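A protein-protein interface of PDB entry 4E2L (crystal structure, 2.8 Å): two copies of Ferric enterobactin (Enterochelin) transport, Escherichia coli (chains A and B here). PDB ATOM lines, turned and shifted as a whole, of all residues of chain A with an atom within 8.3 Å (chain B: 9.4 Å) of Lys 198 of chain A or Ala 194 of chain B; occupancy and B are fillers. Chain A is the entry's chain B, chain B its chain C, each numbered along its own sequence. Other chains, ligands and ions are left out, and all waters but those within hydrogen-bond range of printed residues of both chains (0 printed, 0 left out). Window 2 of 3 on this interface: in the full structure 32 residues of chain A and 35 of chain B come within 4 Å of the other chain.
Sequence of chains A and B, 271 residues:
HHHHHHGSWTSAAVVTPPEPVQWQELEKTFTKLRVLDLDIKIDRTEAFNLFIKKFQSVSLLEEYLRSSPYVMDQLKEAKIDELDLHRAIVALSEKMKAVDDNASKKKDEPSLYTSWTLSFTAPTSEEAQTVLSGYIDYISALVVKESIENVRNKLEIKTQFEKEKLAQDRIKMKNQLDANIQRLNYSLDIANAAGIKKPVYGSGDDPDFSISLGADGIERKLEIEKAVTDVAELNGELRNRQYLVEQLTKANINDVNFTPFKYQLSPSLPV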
ATOM      1  N   ALA A 191     -15.660 -19.861 -13.152  1.00  0.00           N
ATOM      2  CA  ALA A 191     -16.554 -18.784 -12.704  1.00  0.00           C
ATOM      3  C   ALA A 191     -16.834 -17.793 -13.846  1.00  0.00           C
ATOM      4  O   ALA A 191     -17.970 -17.359 -14.044  1.00  0.00           O
ATOM      5  CB  ALA A 191     -15.980 -18.058 -11.482  1.00  0.00           C
ATOM      6  N   ASN A 192     -15.789 -17.451 -14.601  1.00  0.00           N
ATOM      7  CA  ASN A 192     -15.905 -16.549 -15.743  1.00  0.00           C
ATOM      8  C   ASN A 192     -16.608 -17.165 -16.943  1.00  0.00           C
ATOM      9  O   ASN A 192     -17.185 -16.456 -17.745  1.00  0.00           O
ATOM     10  CB  ASN A 192     -14.531 -16.049 -16.177  1.00  0.00           C
ATOM     11  CG  ASN A 192     -13.954 -15.029 -15.220  1.00  0.00           C
ATOM     12  OD1 ASN A 192     -14.692 -14.362 -14.491  1.00  0.00           O
ATOM     13  ND2 ASN A 192     -12.624 -14.892 -15.221  1.00  0.00           N
ATOM     14  N   GLY A 195     -20.211 -16.804 -16.055  1.00  0.00           N
ATOM     15  CA  GLY A 195     -20.597 -15.443 -15.748  1.00  0.00           C
ATOM     16  C   GLY A 195     -21.151 -15.256 -14.352  1.00  0.00           C
ATOM     17  O   GLY A 195     -22.175 -14.590 -14.168  1.00  0.00           O
ATOM     18  N   ILE A 196     -20.492 -15.858 -13.370  1.00  0.00           N
ATOM     19  CA  ILE A 196     -20.771 -15.543 -11.980  1.00  0.00           C
ATOM     20  C   ILE A 196     -19.612 -14.712 -11.469  1.00  0.00           C
ATOM     21  O   ILE A 196     -18.505 -15.217 -11.287  1.00  0.00           O
ATOM     22  CB  ILE A 196     -20.877 -16.798 -11.133  1.00  0.00           C
ATOM     23  CG1 ILE A 196     -21.395 -17.953 -11.986  1.00  0.00           C
ATOM     24  CG2 ILE A 196     -21.747 -16.538  -9.908  1.00  0.00           C
ATOM     25  CD1 ILE A 196     -21.588 -19.215 -11.208  1.00  0.00           C
ATOM     26  N   LYS A 197     -19.857 -13.428 -11.260  1.00  0.00           N
ATOM     27  CA  LYS A 197     -18.773 -12.520 -10.925  1.00  0.00           C
ATOM     28  C   LYS A 197     -18.972 -11.967  -9.523  1.00  0.00           C
ATOM     29  O   LYS A 197     -18.055 -11.434  -8.922  1.00  0.00           O
ATOM     30  CB  LYS A 197     -18.663 -11.407 -11.974  1.00  0.00           C
ATOM     31  CG  LYS A 197     -17.395 -10.559 -11.901  1.00  0.00           C
ATOM     32  CD  LYS A 197     -17.364  -9.492 -13.005  1.00  0.00           C
ATOM     33  CE  LYS A 197     -17.012 -10.073 -14.386  1.00  0.00           C
ATOM     34  NZ  LYS A 197     -15.574 -10.482 -14.512  1.00  0.00           N
ATOM     35  N   LYS A 198     -20.178 -12.101  -8.998  1.00  0.00           N
ATOM     36  CA  LYS A 198     -20.414 -11.803  -7.593  1.00  0.00           C
ATOM     37  C   LYS A 198     -20.829 -13.113  -6.915  1.00  0.00           C
ATOM     38  O   LYS A 198     -21.172 -14.081  -7.607  1.00  0.00           O
ATOM     39  CB  LYS A 198     -21.460 -10.691  -7.428  1.00  0.00           C
ATOM     40  CG  LYS A 198     -20.881  -9.271  -7.492  1.00  0.00           C
ATOM     41  CD  LYS A 198     -19.890  -9.102  -8.655  1.00  0.00           C
ATOM     42  CE  LYS A 198     -20.054  -7.751  -9.383  1.00  0.00           C
ATOM     43  NZ  LYS A 198     -19.249  -7.622 -10.647  1.00  0.00           N
ATOM     44  N   PRO A 199     -20.755 -13.160  -5.569  1.00  0.00           N
ATOM     45  CA  PRO A 199     -21.067 -14.342  -4.752  1.00  0.00           C
ATOM     46  C   PRO A 199     -22.351 -15.082  -5.154  1.00  0.00           C
ATOM     47  O   PRO A 199     -22.986 -14.750  -6.155  1.00  0.00           O
ATOM     48  CB  PRO A 199     -21.214 -13.754  -3.351  1.00  0.00           C
ATOM     49  CG  PRO A 199     -20.273 -12.611  -3.345  1.00  0.00           C
ATOM     50  CD  PRO A 199     -20.247 -12.046  -4.745  1.00  0.00           C
ATOM     51  N   VAL A 200     -22.721 -16.091  -4.372  1.00  0.00           N
ATOM     52  CA  VAL A 200     -23.948 -16.847  -4.607  1.00  0.00           C
ATOM     53  C   VAL A 200     -24.727 -17.070  -3.307  1.00  0.00           C
ATOM     54  O   VAL A 200     -24.259 -17.755  -2.389  1.00  0.00           O
ATOM     55  CB  VAL A 200     -23.660 -18.202  -5.284  1.00  0.00           C
ATOM     56  CG1 VAL A 200     -24.844 -19.144  -5.127  1.00  0.00           C
ATOM     57  CG2 VAL A 200     -23.335 -17.992  -6.747  1.00  0.00           C
ATOM     58  N   ILE A 211     -17.242 -22.479  -7.148  1.00  0.00           N
ATOM     59  CA  ILE A 211     -17.447 -21.245  -7.896  1.00  0.00           C
ATOM     60  C   ILE A 211     -18.186 -20.195  -7.053  1.00  0.00           C
ATOM     61  O   ILE A 211     -18.115 -19.004  -7.326  1.00  0.00           O
ATOM     62  CB  ILE A 211     -18.245 -21.561  -9.158  1.00  0.00           C
ATOM     63  CG1 ILE A 211     -17.346 -22.204 -10.198  1.00  0.00           C
ATOM     64  CG2 ILE A 211     -18.860 -20.324  -9.733  1.00  0.00           C
ATOM     65  CD1 ILE A 211     -18.107 -22.704 -11.421  1.00  0.00           C
ATOM     66  N   SER A 212     -18.888 -20.664  -6.025  1.00  0.00           N
ATOM     67  CA  SER A 212     -19.682 -19.812  -5.149  1.00  0.00           C
ATOM     68  C   SER A 212     -19.150 -18.387  -5.050  1.00  0.00           C
ATOM     69  O   SER A 212     -19.728 -17.471  -5.610  1.00  0.00           O
ATOM     70  CB  SER A 212     -19.778 -20.418  -3.746  1.00  0.00           C
ATOM     71  OG  SER A 212     -18.523 -20.376  -3.076  1.00  0.00           O
ATOM     72  N   LEU A 213     -18.037 -18.202  -4.347  1.00  0.00           N
ATOM     73  CA  LEU A 213     -17.467 -16.867  -4.125  1.00  0.00           C
ATOM     74  C   LEU A 213     -17.613 -15.930  -5.349  1.00  0.00           C
ATOM     75  O   LEU A 213     -17.725 -14.699  -5.218  1.00  0.00           O
ATOM     76  CB  LEU A 213     -16.001 -17.005  -3.710  1.00  0.00           C
ATOM     77  CG  LEU A 213     -15.275 -15.727  -3.361  1.00  0.00           C
ATOM     78  CD1 LEU A 213     -16.029 -15.039  -2.232  1.00  0.00           C
ATOM     79  CD2 LEU A 213     -13.817 -15.969  -2.993  1.00  0.00           C
ATOM     80  N   GLY A 214     -17.620 -16.525  -6.540  1.00  0.00           N
ATOM     81  CA  GLY A 214     -17.707 -15.766  -7.774  1.00  0.00           C
ATOM     82  C   GLY A 214     -16.420 -15.102  -8.234  1.00  0.00           C
ATOM     83  O   GLY A 214     -15.589 -14.672  -7.433  1.00  0.00           O
ATOM     84  N   ALA A 215     -16.287 -14.996  -9.551  1.00  0.00           N
ATOM     85  CA  ALA A 215     -15.081 -14.494 -10.207  1.00  0.00           C
ATOM     86  C   ALA A 215     -14.377 -13.294  -9.545  1.00  0.00           C
ATOM     87  O   ALA A 215     -13.175 -13.112  -9.721  1.00  0.00           O
ATOM     88  CB  ALA A 215     -15.370 -14.201 -11.683  1.00  0.00           C
ATOM     89  N   ASP A 216     -15.105 -12.484  -8.783  1.00  0.00           N
ATOM     90  CA  ASP A 216     -14.506 -11.314  -8.130  1.00  0.00           C
ATOM     91  C   ASP A 216     -13.705 -11.662  -6.870  1.00  0.00           C
ATOM     92  O   ASP A 216     -12.573 -11.209  -6.711  1.00  0.00           O
ATOM     93  CB  ASP A 216     -15.573 -10.268  -7.779  1.00  0.00           C
ATOM     94  CG  ASP A 216     -15.901  -9.331  -8.944  1.00  0.00           C
ATOM     95  OD1 ASP A 216     -15.211  -9.386  -9.993  1.00  0.00           O
ATOM     96  OD2 ASP A 216     -16.847  -8.522  -8.791  1.00  0.00           O
ATOM     97  N   GLY A 217     -14.313 -12.435  -5.969  1.00  0.00           N
ATOM     98  CA  GLY A 217     -13.623 -12.903  -4.782  1.00  0.00           C
ATOM     99  C   GLY A 217     -12.516 -13.893  -5.131  1.00  0.00           C
ATOM    100  O   GLY A 217     -11.356 -13.689  -4.776  1.00  0.00           O
ATOM    101  N   ILE A 218     -12.878 -14.965  -5.831  1.00  0.00           N
ATOM    102  CA  ILE A 218     -11.921 -15.941  -6.339  1.00  0.00           C
ATOM    103  C   ILE A 218     -10.686 -15.296  -6.957  1.00  0.00           C
ATOM    104  O   ILE A 218      -9.664 -15.957  -7.114  1.00  0.00           O
ATOM    105  CB  ILE A 218     -12.581 -16.840  -7.414  1.00  0.00           C
ATOM    106  CG1 ILE A 218     -13.599 -17.777  -6.774  1.00  0.00           C
ATOM    107  CG2 ILE A 218     -11.545 -17.634  -8.196  1.00  0.00           C
ATOM    108  CD1 ILE A 218     -14.310 -18.645  -7.775  1.00  0.00           C
ATOM    109  N   GLU A 219     -10.767 -14.014  -7.312  1.00  0.00           N
ATOM    110  CA  GLU A 219      -9.615 -13.329  -7.920  1.00  0.00           C
ATOM    111  C   GLU A 219      -8.679 -12.686  -6.887  1.00  0.00           C
ATOM    112  O   GLU A 219      -7.448 -12.819  -6.974  1.00  0.00           O
ATOM    113  CB  GLU A 219     -10.069 -12.300  -8.963  1.00  0.00           C
ATOM    114  CG  GLU A 219      -8.943 -11.653  -9.794  1.00  0.00           C
ATOM    115  CD  GLU A 219      -9.368 -10.318 -10.403  1.00  0.00           C
ATOM    116  OE1 GLU A 219      -9.177  -9.285  -9.723  1.00  0.00           O
ATOM    117  OE2 GLU A 219      -9.893 -10.301 -11.545  1.00  0.00           O
ATOM    118  N   ARG A 220      -9.258 -11.987  -5.916  1.00  0.00           N
ATOM    119  CA  ARG A 220      -8.461 -11.402  -4.841  1.00  0.00           C
ATOM    120  C   ARG A 220      -7.861 -12.536  -4.001  1.00  0.00           C
ATOM    121  O   ARG A 220      -6.721 -12.460  -3.530  1.00  0.00           O
ATOM    122  CB  ARG A 220      -9.319 -10.463  -3.985  1.00  0.00           C
ATOM    123  CG  ARG A 220      -8.554  -9.679  -2.921  1.00  0.00           C
ATOM    124  CD  ARG A 220      -7.518  -8.720  -3.522  1.00  0.00           C
ATOM    125  NE  ARG A 220      -6.718  -8.041  -2.496  1.00  0.00           N
ATOM    126  CZ  ARG A 220      -5.492  -8.409  -2.119  1.00  0.00           C
ATOM    127  NH1 ARG A 220      -4.894  -9.453  -2.683  1.00  0.00           N
ATOM    128  NH2 ARG A 220      -4.851  -7.728  -1.179  1.00  0.00           N
ATOM    129  N   SER B 187      -9.611 -11.586   4.750  1.00  0.00           N
ATOM    130  CA  SER B 187     -11.045 -11.656   4.486  1.00  0.00           C
ATOM    131  C   SER B 187     -11.559 -10.247   4.204  1.00  0.00           C
ATOM    132  O   SER B 187     -12.402 -10.032   3.331  1.00  0.00           O
ATOM    133  CB  SER B 187     -11.795 -12.308   5.654  1.00  0.00           C
ATOM    134  OG  SER B 187     -11.738 -13.722   5.563  1.00  0.00           O
ATOM    135  N   LEU B 188     -11.017  -9.290   4.946  1.00  0.00           N
ATOM    136  CA  LEU B 188     -11.266  -7.887   4.695  1.00  0.00           C
ATOM    137  C   LEU B 188     -11.018  -7.548   3.233  1.00  0.00           C
ATOM    138  O   LEU B 188     -11.800  -6.828   2.634  1.00  0.00           O
ATOM    139  CB  LEU B 188     -10.375  -7.020   5.573  1.00  0.00           C
ATOM    140  CG  LEU B 188     -10.732  -5.548   5.449  1.00  0.00           C
ATOM    141  CD1 LEU B 188     -12.223  -5.408   5.670  1.00  0.00           C
ATOM    142  CD2 LEU B 188      -9.947  -4.715   6.443  1.00  0.00           C
ATOM    143  N   ASP B 189      -9.942  -8.070   2.657  1.00  0.00           N
ATOM    144  CA  ASP B 189      -9.644  -7.825   1.246  1.00  0.00           C
ATOM    145  C   ASP B 189     -10.536  -8.597   0.260  1.00  0.00           C
ATOM    146  O   ASP B 189     -10.913  -8.055  -0.776  1.00  0.00           O
ATOM    147  CB  ASP B 189      -8.163  -8.070   0.946  1.00  0.00           C
ATOM    148  CG  ASP B 189      -7.251  -7.068   1.646  1.00  0.00           C
ATOM    149  OD1 ASP B 189      -7.713  -5.933   1.909  1.00  0.00           O
ATOM    150  OD2 ASP B 189      -6.076  -7.418   1.934  1.00  0.00           O
ATOM    151  N   ILE B 190     -10.877  -9.847   0.567  1.00  0.00           N
ATOM    152  CA  ILE B 190     -11.755 -10.604  -0.325  1.00  0.00           C
ATOM    153  C   ILE B 190     -13.186 -10.104  -0.227  1.00  0.00           C
ATOM    154  O   ILE B 190     -13.916 -10.078  -1.224  1.00  0.00           O
ATOM    155  CB  ILE B 190     -11.726 -12.122  -0.078  1.00  0.00           C
ATOM    156  CG1 ILE B 190     -10.572 -12.760  -0.848  1.00  0.00           C
ATOM    157  CG2 ILE B 190     -13.028 -12.763  -0.538  1.00  0.00           C
ATOM    158  CD1 ILE B 190      -9.479 -13.284   0.020  1.00  0.00           C
ATOM    159  N   ALA B 191     -13.593  -9.705   0.975  1.00  0.00           N
ATOM    160  CA  ALA B 191     -14.878  -9.028   1.138  1.00  0.00           C
ATOM    161  C   ALA B 191     -14.971  -7.854   0.145  1.00  0.00           C
ATOM    162  O   ALA B 191     -15.773  -7.877  -0.787  1.00  0.00           O
ATOM    163  CB  ALA B 191     -15.055  -8.547   2.581  1.00  0.00           C
ATOM    164  N   ASN B 192     -14.125  -6.848   0.359  1.00  0.00           N
ATOM    165  CA  ASN B 192     -13.981  -5.702  -0.531  1.00  0.00           C
ATOM    166  C   ASN B 192     -14.053  -6.031  -2.025  1.00  0.00           C
ATOM    167  O   ASN B 192     -14.985  -5.617  -2.696  1.00  0.00           O
ATOM    168  CB  ASN B 192     -12.690  -4.925  -0.222  1.00  0.00           C
ATOM    169  CG  ASN B 192     -12.766  -4.146   1.088  1.00  0.00           C
ATOM    170  OD1 ASN B 192     -13.857  -3.858   1.594  1.00  0.00           O
ATOM    171  ND2 ASN B 192     -11.602  -3.798   1.643  1.00  0.00           N
ATOM    172  N   ALA B 193     -13.082  -6.764  -2.558  1.00  0.00           N
ATOM    173  CA  ALA B 193     -13.066  -7.057  -3.993  1.00  0.00           C
ATOM    174  C   ALA B 193     -14.314  -7.779  -4.543  1.00  0.00           C
ATOM    175  O   ALA B 193     -14.482  -7.857  -5.756  1.00  0.00           O
ATOM    176  CB  ALA B 193     -11.797  -7.814  -4.377  1.00  0.00           C
ATOM    177  N   ALA B 194     -15.186  -8.306  -3.680  1.00  0.00           N
ATOM    178  CA  ALA B 194     -16.434  -8.926  -4.158  1.00  0.00           C
ATOM    179  C   ALA B 194     -17.655  -8.001  -4.038  1.00  0.00           C
ATOM    180  O   ALA B 194     -18.779  -8.390  -4.381  1.00  0.00           O
ATOM    181  CB  ALA B 194     -16.699 -10.245  -3.453  1.00  0.00           C
ATOM    182  N   GLY B 195     -17.426  -6.781  -3.555  1.00  0.00           N
ATOM    183  CA  GLY B 195     -18.481  -5.801  -3.381  1.00  0.00           C
ATOM    184  C   GLY B 195     -19.213  -5.901  -2.049  1.00  0.00           C
ATOM    185  O   GLY B 195     -19.804  -4.919  -1.579  1.00  0.00           O
ATOM    186  N   ILE B 196     -19.172  -7.082  -1.429  1.00  0.00           N
ATOM    187  CA  ILE B 196     -19.952  -7.333  -0.219  1.00  0.00           C
ATOM    188  C   ILE B 196     -19.577  -6.449   0.957  1.00  0.00           C
ATOM    189  O   ILE B 196     -18.704  -6.798   1.755  1.00  0.00           O
ATOM    190  CB  ILE B 196     -19.835  -8.770   0.222  1.00  0.00           C
ATOM    191  CG1 ILE B 196     -20.125  -9.684  -0.964  1.00  0.00           C
ATOM    192  CG2 ILE B 196     -20.793  -9.025   1.374  1.00  0.00           C
ATOM    193  CD1 ILE B 196     -20.656 -11.036  -0.549  1.00  0.00           C
ATOM    194  N   LYS B 197     -20.249  -5.305   1.055  1.00  0.00           N
ATOM    195  CA  LYS B 197     -19.978  -4.347   2.114  1.00  0.00           C
ATOM    196  C   LYS B 197     -20.819  -4.676   3.356  1.00  0.00           C
ATOM    197  O   LYS B 197     -20.289  -4.703   4.461  1.00  0.00           O
ATOM    198  CB  LYS B 197     -20.215  -2.910   1.632  1.00  0.00           C
ATOM    199  N   LYS B 198     -22.107  -4.964   3.181  1.00  0.00           N
ATOM    200  CA  LYS B 198     -22.945  -5.274   4.336  1.00  0.00           C
ATOM    201  C   LYS B 198     -23.193  -6.772   4.539  1.00  0.00           C
ATOM    202  O   LYS B 198     -23.040  -7.568   3.613  1.00  0.00           O
ATOM    203  CB  LYS B 198     -24.268  -4.500   4.304  1.00  0.00           C
ATOM    204  CG  LYS B 198     -24.201  -3.148   4.990  1.00  0.00           C
ATOM    205  N   PHE B 209     -11.684 -18.203   3.948  1.00  0.00           N
ATOM    206  CA  PHE B 209     -11.785 -16.806   4.365  1.00  0.00           C
ATOM    207  C   PHE B 209     -13.244 -16.343   4.333  1.00  0.00           C
ATOM    208  O   PHE B 209     -13.671 -15.723   3.357  1.00  0.00           O
ATOM    209  CB  PHE B 209     -10.987 -15.887   3.431  1.00  0.00           C
ATOM    210  CG  PHE B 209      -9.578 -16.339   3.148  1.00  0.00           C
ATOM    211  CD1 PHE B 209      -9.314 -17.242   2.126  1.00  0.00           C
ATOM    212  CD2 PHE B 209      -8.507 -15.814   3.861  1.00  0.00           C
ATOM    213  CE1 PHE B 209      -8.011 -17.638   1.842  1.00  0.00           C
ATOM    214  CE2 PHE B 209      -7.198 -16.208   3.583  1.00  0.00           C
ATOM    215  CZ  PHE B 209      -6.953 -17.119   2.571  1.00  0.00           C
ATOM    216  N   ILE B 211     -16.552 -14.305   4.415  1.00  0.00           N
ATOM    217  CA  ILE B 211     -16.847 -12.880   4.190  1.00  0.00           C
ATOM    218  C   ILE B 211     -18.284 -12.525   4.595  1.00  0.00           C
ATOM    219  O   ILE B 211     -18.644 -11.351   4.620  1.00  0.00           O
ATOM    220  CB  ILE B 211     -16.625 -12.480   2.724  1.00  0.00           C
ATOM    221  CG1 ILE B 211     -17.202 -13.550   1.797  1.00  0.00           C
ATOM    222  CG2 ILE B 211     -15.147 -12.306   2.439  1.00  0.00           C
ATOM    223  CD1 ILE B 211     -16.809 -13.352   0.348  1.00  0.00           C
ATOM    224  N   SER B 212     -19.079 -13.547   4.913  1.00  0.00           N
ATOM    225  CA  SER B 212     -20.426 -13.385   5.442  1.00  0.00           C
ATOM    226  C   SER B 212     -20.695 -12.033   6.073  1.00  0.00           C
ATOM    227  O   SER B 212     -21.565 -11.297   5.628  1.00  0.00           O
ATOM    228  CB  SER B 212     -20.714 -14.463   6.473  1.00  0.00           C
ATOM    229  OG  SER B 212     -20.444 -15.746   5.970  1.00  0.00           O
ATOM    230  N   GLY B 214     -19.472  -9.280   5.931  1.00  0.00           N
ATOM    231  CA  GLY B 214     -19.319  -8.091   5.113  1.00  0.00           C
ATOM    232  C   GLY B 214     -18.321  -7.078   5.651  1.00  0.00           C
ATOM    233  O   GLY B 214     -18.168  -6.910   6.865  1.00  0.00           O
ATOM    234  N   ALA B 215     -17.674  -6.376   4.723  1.00  0.00           N
ATOM    235  CA  ALA B 215     -16.547  -5.484   5.007  1.00  0.00           C
ATOM    236  C   ALA B 215     -16.676  -4.508   6.193  1.00  0.00           C
ATOM    237  O   ALA B 215     -15.700  -4.292   6.910  1.00  0.00           O
ATOM    238  CB  ALA B 215     -16.128  -4.732   3.735  1.00  0.00           C
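Of the 17 printed residues of chain B, 5 touch a printed residue of chain A.
Printed residues of chain B that touch a printed residue of chain A: Asp 189, Ala 193, Ala 194, Ile 196 and Ile 211.
Hydrophobic or aromatic side chains of chain B within 4 Å of the printed part of chain A: Ala 193, Ile 196 and Ile 211.
Along chain B the printed residues that touch a printed residue of chain A span positions 189 to 211.
Of the 18 printed residues of chain A, 5 touch a printed residue of chain B.
Along chain A the printed residues that touch a printed residue of chain B span positions 198 to 220.
Among the printed residues, 8 pairs touch across the chains.
Positions printed for both chains: 191, 192, 195, 196, 197, 198, 211, 212, 214 and 215.
Of the 8 pairs that touch across the chains among the printed residues, none has its exchanged pair printed and touching as well.
The backbone carbonyl oxygen of Ile 196 of chain B lies within hydrogen-bond range of the backbone NH of Ala 215 of chain B, 3.2 Å away.
NZ of Lys 198 of chain A is in salt-bridge range of OD2 of Asp 216 of chain A, at 3.2 Å.
The backbone carbonyl oxygen (O) of Lys 197 of chain A lies close to the backbone NH (N) of Asp 216 of chain A (3.1 Å).
Lys 198 of chain A touches one residue of chain B.
Of chain A, only Lys 198, Pro 199 and Asp 216 come within 4 Å of Ala 194 of chain B.
Pro 199 of chain A touches just these residues of chain B: Ala 194 (3.96 Å) and Ile 196 (3.2 Å).
Asp 216 of chain A touches just these residues of chain B: Ala 193 (3.3 Å) and Ala 194 (3.96 Å).
Of the printed residues of chain A, Ile 196 of chain B touches Pro 199 (3.2 Å).
Printed residues of chain A within 4 Å of Ile 211 of chain B: Leu 213 (3.2 Å).
Leu 188 of chain B touches none of the printed residues of chain A.
Lys 198 of chain B touches none of the printed residues of chain A.
The nearest residue of chain B that does not touch Lys 198 of chain A is Gly 195 of chain B (5.8 Å).
The nearest printed residue of chain A that does not touch Ile 196 of chain B is Leu 213 of chain A (6.3 Å).
Among the printed residues, merely in contact across the chains: Leu 213 of chain A with Ile 211 of chain B, Pro 199 of chain A with Ile 196 of chain B, Asp 216 of chain A with Ala 193 of chain B, Arg 220 of chain A with Ala 193 of chain B, Lys 198 of chain A with Ala 194 of chain B, Pro 199 of chain A with Ala 194 of chain B and Asp 216 of chain A with Ala 194 of chain B.
The guanidinium group (NH2) of Arg 220 of chain A lies within salt-bridge range of the side-chain carboxylate (OD2) of Asp 189 of chain B.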
